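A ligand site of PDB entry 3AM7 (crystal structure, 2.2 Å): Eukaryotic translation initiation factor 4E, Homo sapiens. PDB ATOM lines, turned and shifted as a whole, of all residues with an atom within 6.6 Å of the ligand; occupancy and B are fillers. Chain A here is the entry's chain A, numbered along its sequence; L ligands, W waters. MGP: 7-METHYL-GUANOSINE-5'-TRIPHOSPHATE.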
ATOM      1  N   PHE A  22       2.701   5.768 -13.347  1.00  0.00           N
ATOM      2  CA  PHE A  22       1.338   5.254 -13.305  1.00  0.00           C
ATOM      3  C   PHE A  22       0.713   5.506 -11.939  1.00  0.00           C
ATOM      4  O   PHE A  22       1.260   5.127 -10.906  1.00  0.00           O
ATOM      5  CB  PHE A  22       1.331   3.746 -13.602  1.00  0.00           C
ATOM      6  CG  PHE A  22      -0.030   3.135 -13.484  1.00  0.00           C
ATOM      7  CD1 PHE A  22      -0.887   3.092 -14.581  1.00  0.00           C
ATOM      8  CD2 PHE A  22      -0.475   2.624 -12.277  1.00  0.00           C
ATOM      9  CE1 PHE A  22      -2.157   2.558 -14.473  1.00  0.00           C
ATOM     10  CE2 PHE A  22      -1.747   2.087 -12.159  1.00  0.00           C
ATOM     11  CZ  PHE A  22      -2.591   2.048 -13.254  1.00  0.00           C
ATOM     12  N   THR A  29      -9.546   4.027 -16.903  1.00  0.00           N
ATOM     13  CA  THR A  29      -8.978   2.913 -17.653  1.00  0.00           C
ATOM     14  C   THR A  29      -7.496   2.866 -17.285  1.00  0.00           C
ATOM     15  O   THR A  29      -6.911   3.880 -16.931  1.00  0.00           O
ATOM     16  CB  THR A  29      -9.100   3.132 -19.173  1.00  0.00           C
ATOM     17  OG1 THR A  29     -10.481   3.111 -19.551  1.00  0.00           O
ATOM     18  CG2 THR A  29      -8.365   2.048 -19.939  1.00  0.00           C
ATOM     19  N   TRP A  30      -6.901   1.685 -17.349  1.00  0.00           N
ATOM     20  CA  TRP A  30      -5.486   1.543 -17.017  1.00  0.00           C
ATOM     21  C   TRP A  30      -4.642   2.545 -17.815  1.00  0.00           C
ATOM     22  O   TRP A  30      -3.808   3.246 -17.236  1.00  0.00           O
ATOM     23  CB  TRP A  30      -5.014   0.115 -17.304  1.00  0.00           C
ATOM     24  CG  TRP A  30      -3.559  -0.084 -16.964  1.00  0.00           C
ATOM     25  CD1 TRP A  30      -3.051  -0.397 -15.737  1.00  0.00           C
ATOM     26  CD2 TRP A  30      -2.443   0.062 -17.845  1.00  0.00           C
ATOM     27  NE1 TRP A  30      -1.686  -0.446 -15.802  1.00  0.00           N
ATOM     28  CE2 TRP A  30      -1.285  -0.167 -17.083  1.00  0.00           C
ATOM     29  CE3 TRP A  30      -2.318   0.371 -19.198  1.00  0.00           C
ATOM     30  CZ2 TRP A  30      -0.002  -0.092 -17.622  1.00  0.00           C
ATOM     31  CZ3 TRP A  30      -1.034   0.448 -19.747  1.00  0.00           C
ATOM     32  CH2 TRP A  30       0.104   0.219 -18.955  1.00  0.00           C
ATOM     33  N   GLN A  31      -4.848   2.611 -19.117  1.00  0.00           N
ATOM     34  CA  GLN A  31      -4.095   3.519 -19.984  1.00  0.00           C
ATOM     35  C   GLN A  31      -4.231   4.998 -19.605  1.00  0.00           C
ATOM     36  O   GLN A  31      -3.274   5.761 -19.740  1.00  0.00           O
ATOM     37  CB  GLN A  31      -4.507   3.322 -21.450  1.00  0.00           C
ATOM     38  CG  GLN A  31      -3.632   4.098 -22.438  1.00  0.00           C
ATOM     39  CD  GLN A  31      -3.978   3.808 -23.894  1.00  0.00           C
ATOM     40  OE1 GLN A  31      -5.083   4.080 -24.355  1.00  0.00           O
ATOM     41  NE2 GLN A  31      -3.011   3.241 -24.627  1.00  0.00           N
ATOM     42  N   GLY A  62       0.436   1.079  -5.420  1.00  0.00           N
ATOM     43  CA  GLY A  62      -0.432   1.134  -6.583  1.00  0.00           C
ATOM     44  C   GLY A  62       0.130   1.962  -7.725  1.00  0.00           C
ATOM     45  O   GLY A  62      -0.514   2.110  -8.763  1.00  0.00           O
ATOM     46  N   ASP A  64       3.432   2.953 -10.490  1.00  0.00           N
ATOM     47  CA  ASP A  64       4.503   2.303 -11.227  1.00  0.00           C
ATOM     48  C   ASP A  64       5.411   3.335 -11.862  1.00  0.00           C
ATOM     49  O   ASP A  64       5.009   4.462 -12.141  1.00  0.00           O
ATOM     50  CB  ASP A  64       3.996   1.427 -12.382  1.00  0.00           C
ATOM     51  CG  ASP A  64       2.946   0.419 -11.984  1.00  0.00           C
ATOM     52  OD1 ASP A  64       3.015  -0.141 -10.876  1.00  0.00           O
ATOM     53  OD2 ASP A  64       2.040   0.176 -12.811  1.00  0.00           O
ATOM     54  N   PRO A  74       4.918   1.588 -22.544  1.00  0.00           N
ATOM     55  CA  PRO A  74       5.010   0.538 -21.528  1.00  0.00           C
ATOM     56  C   PRO A  74       3.736  -0.293 -21.331  1.00  0.00           C
ATOM     57  O   PRO A  74       3.221  -0.401 -20.220  1.00  0.00           O
ATOM     58  CB  PRO A  74       5.431   1.316 -20.275  1.00  0.00           C
ATOM     59  CG  PRO A  74       4.687   2.601 -20.436  1.00  0.00           C
ATOM     60  CD  PRO A  74       4.826   2.928 -21.929  1.00  0.00           C
ATOM     61  N   MET A  75       3.260  -0.896 -22.411  1.00  0.00           N
ATOM     62  CA  MET A  75       2.051  -1.719 -22.362  1.00  0.00           C
ATOM     63  C   MET A  75       2.177  -2.940 -23.263  1.00  0.00           C
ATOM     64  O   MET A  75       2.963  -2.952 -24.204  1.00  0.00           O
ATOM     65  CB  MET A  75       0.835  -0.885 -22.749  1.00  0.00           C
ATOM     66  CG  MET A  75       0.854  -0.371 -24.177  1.00  0.00           C
ATOM     67  SD  MET A  75      -0.489   0.780 -24.534  1.00  0.00           S
ATOM     68  CE  MET A  75       0.038   2.188 -23.563  1.00  0.00           C
ATOM     69  N   TRP A  76       1.397  -3.978 -22.952  1.00  0.00           N
ATOM     70  CA  TRP A  76       1.408  -5.244 -23.699  1.00  0.00           C
ATOM     71  C   TRP A  76       1.087  -5.079 -25.162  1.00  0.00           C
ATOM     72  O   TRP A  76       1.675  -5.737 -26.013  1.00  0.00           O
ATOM     73  CB  TRP A  76       0.377  -6.227 -23.135  1.00  0.00           C
ATOM     74  CG  TRP A  76       0.470  -6.548 -21.680  1.00  0.00           C
ATOM     75  CD1 TRP A  76       1.604  -6.826 -20.976  1.00  0.00           C
ATOM     76  CD2 TRP A  76      -0.624  -6.767 -20.787  1.00  0.00           C
ATOM     77  NE1 TRP A  76       1.289  -7.205 -19.695  1.00  0.00           N
ATOM     78  CE2 TRP A  76      -0.075  -7.182 -19.555  1.00  0.00           C
ATOM     79  CE3 TRP A  76      -2.015  -6.663 -20.908  1.00  0.00           C
ATOM     80  CZ2 TRP A  76      -0.872  -7.493 -18.439  1.00  0.00           C
ATOM     81  CZ3 TRP A  76      -2.812  -6.974 -19.792  1.00  0.00           C
ATOM     82  CH2 TRP A  76      -2.235  -7.375 -18.574  1.00  0.00           C
ATOM     83  N   GLU A  77       0.135  -4.209 -25.448  1.00  0.00           N
ATOM     84  CA  GLU A  77      -0.352  -3.958 -26.796  1.00  0.00           C
ATOM     85  C   GLU A  77       0.636  -3.367 -27.777  1.00  0.00           C
ATOM     86  O   GLU A  77       0.417  -3.453 -28.990  1.00  0.00           O
ATOM     87  CB  GLU A  77      -1.593  -3.073 -26.730  1.00  0.00           C
ATOM     88  CG  GLU A  77      -2.676  -3.579 -25.796  1.00  0.00           C
ATOM     89  CD  GLU A  77      -2.640  -2.926 -24.421  1.00  0.00           C
ATOM     90  OE1 GLU A  77      -1.649  -3.133 -23.690  1.00  0.00           O
ATOM     91  OE2 GLU A  77      -3.606  -2.210 -24.083  1.00  0.00           O
ATOM     92  N   ARG A  86       8.532 -10.856 -19.899  1.00  0.00           N
ATOM     93  CA  ARG A  86       9.335 -10.162 -18.895  1.00  0.00           C
ATOM     94  C   ARG A  86       9.967 -11.115 -17.900  1.00  0.00           C
ATOM     95  O   ARG A  86       9.441 -12.195 -17.649  1.00  0.00           O
ATOM     96  CB  ARG A  86       8.451  -9.211 -18.111  1.00  0.00           C
ATOM     97  CG  ARG A  86       7.330  -9.950 -17.356  1.00  0.00           C
ATOM     98  CD  ARG A  86       6.405  -9.036 -16.577  1.00  0.00           C
ATOM     99  NE  ARG A  86       5.441  -9.819 -15.810  1.00  0.00           N
ATOM    100  CZ  ARG A  86       4.650  -9.344 -14.855  1.00  0.00           C
ATOM    101  NH1 ARG A  86       3.817 -10.167 -14.223  1.00  0.00           N
ATOM    102  NH2 ARG A  86       4.677  -8.057 -14.518  1.00  0.00           N
ATOM    103  N   VAL A 127       9.867  -2.222 -15.600  1.00  0.00           N
ATOM    104  CA  VAL A 127       8.840  -1.554 -14.811  1.00  0.00           C
ATOM    105  C   VAL A 127       8.917  -1.982 -13.358  1.00  0.00           C
ATOM    106  O   VAL A 127       9.231  -3.134 -13.054  1.00  0.00           O
ATOM    107  CB  VAL A 127       7.406  -1.838 -15.357  1.00  0.00           C
ATOM    108  CG1 VAL A 127       7.387  -3.095 -16.158  1.00  0.00           C
ATOM    109  CG2 VAL A 127       6.402  -1.934 -14.208  1.00  0.00           C
ATOM    110  N   ASN A 129       6.652  -2.034  -9.911  1.00  0.00           N
ATOM    111  CA  ASN A 129       5.324  -1.875  -9.348  1.00  0.00           C
ATOM    112  C   ASN A 129       5.447  -1.735  -7.824  1.00  0.00           C
ATOM    113  O   ASN A 129       6.014  -2.611  -7.159  1.00  0.00           O
ATOM    114  CB  ASN A 129       4.438  -3.090  -9.646  1.00  0.00           C
ATOM    115  CG  ASN A 129       4.375  -3.411 -11.135  1.00  0.00           C
ATOM    116  OD1 ASN A 129       4.786  -4.485 -11.552  1.00  0.00           O
ATOM    117  ND2 ASN A 129       3.848  -2.486 -11.928  1.00  0.00           N
ATOM    118  N   ARG A 131       3.636  -2.074  -4.574  1.00  0.00           N
ATOM    119  CA  ARG A 131       2.387  -2.688  -4.100  1.00  0.00           C
ATOM    120  C   ARG A 131       2.438  -3.032  -2.624  1.00  0.00           C
ATOM    121  O   ARG A 131       3.483  -3.414  -2.097  1.00  0.00           O
ATOM    122  CB  ARG A 131       2.100  -3.947  -4.928  1.00  0.00           C
ATOM    123  CG  ARG A 131       1.939  -3.696  -6.422  1.00  0.00           C
ATOM    124  CD  ARG A 131       0.569  -3.082  -6.733  1.00  0.00           C
ATOM    125  NE  ARG A 131       0.362  -2.910  -8.171  1.00  0.00           N
ATOM    126  CZ  ARG A 131       0.907  -1.939  -8.904  1.00  0.00           C
ATOM    127  NH1 ARG A 131       1.691  -1.037  -8.332  1.00  0.00           N
ATOM    128  NH2 ARG A 131       0.688  -1.898 -10.215  1.00  0.00           N
ATOM    129  N   LYS A 133       1.067  -5.574  -1.189  1.00  0.00           N
ATOM    130  CA  LYS A 133       1.246  -7.008  -0.994  1.00  0.00           C
ATOM    131  C   LYS A 133       2.655  -7.459  -1.364  1.00  0.00           C
ATOM    132  O   LYS A 133       3.052  -8.577  -1.041  1.00  0.00           O
ATOM    133  CB  LYS A 133       0.219  -7.794  -1.828  1.00  0.00           C
ATOM    134  CG  LYS A 133       0.536  -7.820  -3.315  1.00  0.00           C
ATOM    135  CD  LYS A 133      -0.570  -8.471  -4.128  1.00  0.00           C
ATOM    136  CE  LYS A 133      -0.212  -8.528  -5.619  1.00  0.00           C
ATOM    137  NZ  LYS A 133       0.206  -7.201  -6.195  1.00  0.00           N
ATOM    138  N   GLY A 134       3.398  -6.589  -2.044  1.00  0.00           N
ATOM    139  CA  GLY A 134       4.747  -6.954  -2.447  1.00  0.00           C
ATOM    140  C   GLY A 134       5.142  -6.282  -3.747  1.00  0.00           C
ATOM    141  O   GLY A 134       4.429  -6.380  -4.751  1.00  0.00           O
ATOM    142  N   LYS A 136       7.312  -5.391  -7.203  1.00  0.00           N
ATOM    143  CA  LYS A 136       7.796  -6.179  -8.335  1.00  0.00           C
ATOM    144  C   LYS A 136       8.606  -5.331  -9.309  1.00  0.00           C
ATOM    145  O   LYS A 136       8.306  -4.153  -9.541  1.00  0.00           O
ATOM    146  CB  LYS A 136       6.619  -6.797  -9.082  1.00  0.00           C
ATOM    147  CG  LYS A 136       6.134  -8.145  -8.551  1.00  0.00           C
ATOM    148  CD  LYS A 136       4.615  -8.172  -8.389  1.00  0.00           C
ATOM    149  CE  LYS A 136       3.895  -7.696  -9.630  1.00  0.00           C
ATOM    150  NZ  LYS A 136       2.420  -7.588  -9.412  1.00  0.00           N
ATOM    151  N   TRP A 140      11.263  -6.040 -19.524  1.00  0.00           N
ATOM    152  CA  TRP A 140      10.467  -6.520 -20.652  1.00  0.00           C
ATOM    153  C   TRP A 140      11.326  -6.704 -21.900  1.00  0.00           C
ATOM    154  O   TRP A 140      12.153  -5.852 -22.210  1.00  0.00           O
ATOM    155  CB  TRP A 140       9.376  -5.495 -20.959  1.00  0.00           C
ATOM    156  CG  TRP A 140       8.248  -5.435 -19.985  1.00  0.00           C
ATOM    157  CD1 TRP A 140       8.301  -5.716 -18.658  1.00  0.00           C
ATOM    158  CD2 TRP A 140       6.904  -5.053 -20.269  1.00  0.00           C
ATOM    159  NE1 TRP A 140       7.067  -5.523 -18.086  1.00  0.00           N
ATOM    160  CE2 TRP A 140       6.194  -5.113 -19.059  1.00  0.00           C
ATOM    161  CE3 TRP A 140       6.231  -4.649 -21.434  1.00  0.00           C
ATOM    162  CZ2 TRP A 140       4.837  -4.788 -18.963  1.00  0.00           C
ATOM    163  CZ3 TRP A 140       4.884  -4.325 -21.347  1.00  0.00           C
ATOM    164  CH2 TRP A 140       4.199  -4.403 -20.119  1.00  0.00           C
ATOM    165  N   THR A 177      -0.642 -14.082 -19.990  1.00  0.00           N
ATOM    166  CA  THR A 177      -1.184 -13.644 -18.707  1.00  0.00           C
ATOM    167  C   THR A 177      -2.595 -14.184 -18.457  1.00  0.00           C
ATOM    168  O   THR A 177      -3.431 -14.220 -19.371  1.00  0.00           O
ATOM    169  CB  THR A 177      -1.211 -12.102 -18.560  1.00  0.00           C
ATOM    170  OG1 THR A 177      -2.523 -11.601 -18.826  1.00  0.00           O
ATOM    171  CG2 THR A 177      -0.231 -11.458 -19.515  1.00  0.00           C
ATOM    172  N   ALA A 178      -2.842 -14.602 -17.223  1.00  0.00           N
ATOM    173  CA  ALA A 178      -4.134 -15.156 -16.829  1.00  0.00           C
ATOM    174  C   ALA A 178      -5.314 -14.291 -17.255  1.00  0.00           C
ATOM    175  O   ALA A 178      -5.267 -13.059 -17.152  1.00  0.00           O
ATOM    176  CB  ALA A 178      -4.167 -15.376 -15.324  1.00  0.00           C
HETATM  177  PA  MGP L   1      -0.122  -5.222 -12.600  1.00  0.00           P
HETATM  178  O1A MGP L   1       0.001  -3.741 -12.414  1.00  0.00           O
HETATM  179  O2A MGP L   1       0.947  -5.669 -13.549  1.00  0.00           O
HETATM  180  O3A MGP L   1       0.055  -5.977 -11.214  1.00  0.00           O
HETATM  181  O5' MGP L   1      -1.592  -5.573 -13.306  1.00  0.00           O
HETATM  182  PB  MGP L   1      -0.881  -5.768  -9.935  1.00  0.00           P
HETATM  183  O1B MGP L   1      -1.439  -4.388  -9.859  1.00  0.00           O
HETATM  184  O2B MGP L   1      -0.008  -6.073  -8.794  1.00  0.00           O
HETATM  185  O3B MGP L   1      -1.976  -6.723  -9.925  1.00  0.00           O
HETATM  186  PC  MGP L   1      -2.132  -8.312  -9.957  1.00  0.00           P
HETATM  187  O1C MGP L   1      -2.704  -8.482  -8.420  1.00  0.00           O
HETATM  188  O2C MGP L   1      -0.765  -8.942 -10.124  1.00  0.00           O
HETATM  189  O3C MGP L   1      -3.085  -8.998 -10.943  1.00  0.00           O
HETATM  190  C5' MGP L   1      -2.858  -5.057 -12.850  1.00  0.00           C
HETATM  191  C4' MGP L   1      -3.849  -4.821 -13.929  1.00  0.00           C
HETATM  192  O4' MGP L   1      -3.348  -3.655 -14.723  1.00  0.00           O
HETATM  193  C3' MGP L   1      -3.998  -5.856 -15.053  1.00  0.00           C
HETATM  194  O3' MGP L   1      -4.777  -7.036 -14.701  1.00  0.00           O
HETATM  195  C2' MGP L   1      -4.617  -5.054 -16.166  1.00  0.00           C
HETATM  196  O2' MGP L   1      -6.066  -4.938 -15.943  1.00  0.00           O
HETATM  197  C1' MGP L   1      -3.808  -3.772 -16.117  1.00  0.00           C
HETATM  198  N9  MGP L   1      -2.483  -3.729 -16.892  1.00  0.00           N
HETATM  199  C8  MGP L   1      -1.172  -3.861 -16.515  1.00  0.00           C
HETATM  200  N7  MGP L   1      -0.381  -3.758 -17.558  1.00  0.00           N
HETATM  201  CM7 MGP L   1       1.089  -3.854 -17.500  1.00  0.00           C
HETATM  202  C5  MGP L   1      -1.150  -3.506 -18.820  1.00  0.00           C
HETATM  203  C6  MGP L   1      -0.939  -3.324 -20.128  1.00  0.00           C
HETATM  204  O6  MGP L   1       0.243  -3.325 -20.680  1.00  0.00           O
HETATM  205  N1  MGP L   1      -2.140  -3.136 -20.918  1.00  0.00           N
HETATM  206  C2  MGP L   1      -3.463  -3.126 -20.431  1.00  0.00           C
HETATM  207  N2  MGP L   1      -4.464  -2.930 -21.282  1.00  0.00           N
HETATM  208  N3  MGP L   1      -3.697  -3.314 -19.074  1.00  0.00           N
HETATM  209  C4  MGP L   1      -2.514  -3.519 -18.249  1.00  0.00           C
HETATM  210  O   HOH W   1       1.469  -9.598 -12.402  1.00  0.00           O
HETATM  211  O   HOH W   2      -7.377  -1.847 -21.189  1.00  0.00           O
HETATM  212  O   HOH W   3      -6.191  -2.984 -18.169  1.00  0.00           O
HETATM  213  O   HOH W   4      -3.492  -0.108 -22.704  1.00  0.00           O
HETATM  214  O   HOH W   5       3.231  -6.732 -12.472  1.00  0.00           O
HETATM  215  O   HOH W   6       1.421 -10.108  -7.755  1.00  0.00           O
HETATM  216  O   HOH W   7      -5.000  -1.738 -12.593  1.00  0.00           O
HETATM  217  O   HOH W   8       3.482  -4.550 -14.864  1.00  0.00           O
HETATM  218  O   HOH W   9      -4.776  -6.257 -10.017  1.00  0.00           O
HETATM  219  O   HOH W  10       0.061  -1.247 -13.777  1.00  0.00           O
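The side-chain carboxylate of Asp 64 lies within salt-bridge range of the guanidinium group of Arg 131 (3.0 Å).
The backbone NH of Asn 129 is in hydrogen-bond range of the backbone carbonyl oxygen of Lys 136 (2.7 Å).
SD of Met 75 sits close to NE2 of Gln 31 (3.5 Å).
Merely in contact with the ligand: Trp 30 and Met 75.
Seven residues have an atom within 4 Å of the ligand: Trp 30, Met 75, Trp 76, Glu 77, Arg 131, Lys 133 and Lys 136.
An oxygen (O6) of the ligand sits at hydrogen-bond distance from the backbone NH (N) of Trp 76 (2.6 Å).
A nitrogen (N1) of the ligand is in hydrogen-bond range of the side-chain carboxylate of Glu 77 (2.8 Å).
The side-chain amino group (NZ) of Lys 133 lies within salt-bridge range of an oxygen (O2B) of the ligand.
NE of Arg 131 is in salt-bridge range of O1B of the ligand.
The side-chain amino group of Lys 136 lies within salt-bridge range of an oxygen (O2B) of the ligand (2.9 Å).
Water W5 lies within hydrogen-bond range of an oxygen (O2A) of the ligand (2.7 Å), the guanidinium group of Arg 86 (2.8 Å), the side-chain amide oxygen of Asn 129 (2.9 Å) and the side-chain amino group of Lys 136 (3.3 Å).
Water W10 lies within hydrogen-bond range of OD2 of Asp 64, NE1 of Trp 30 and O1A of the ligand.
Water W1 lies within hydrogen-bond range of the guanidinium group (NH1) of Arg 86 and an oxygen (O2C) of the ligand.
Water W4 lies within hydrogen-bond range of the side-chain carboxylate (OE2) of Glu 77, a nitrogen (N2) of the ligand and the side-chain sulfur (SD) of Met 75.
Water W6 bridges NZ of Lys 136 (3.2 Å) and O2C of the ligand (3.4 Å).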
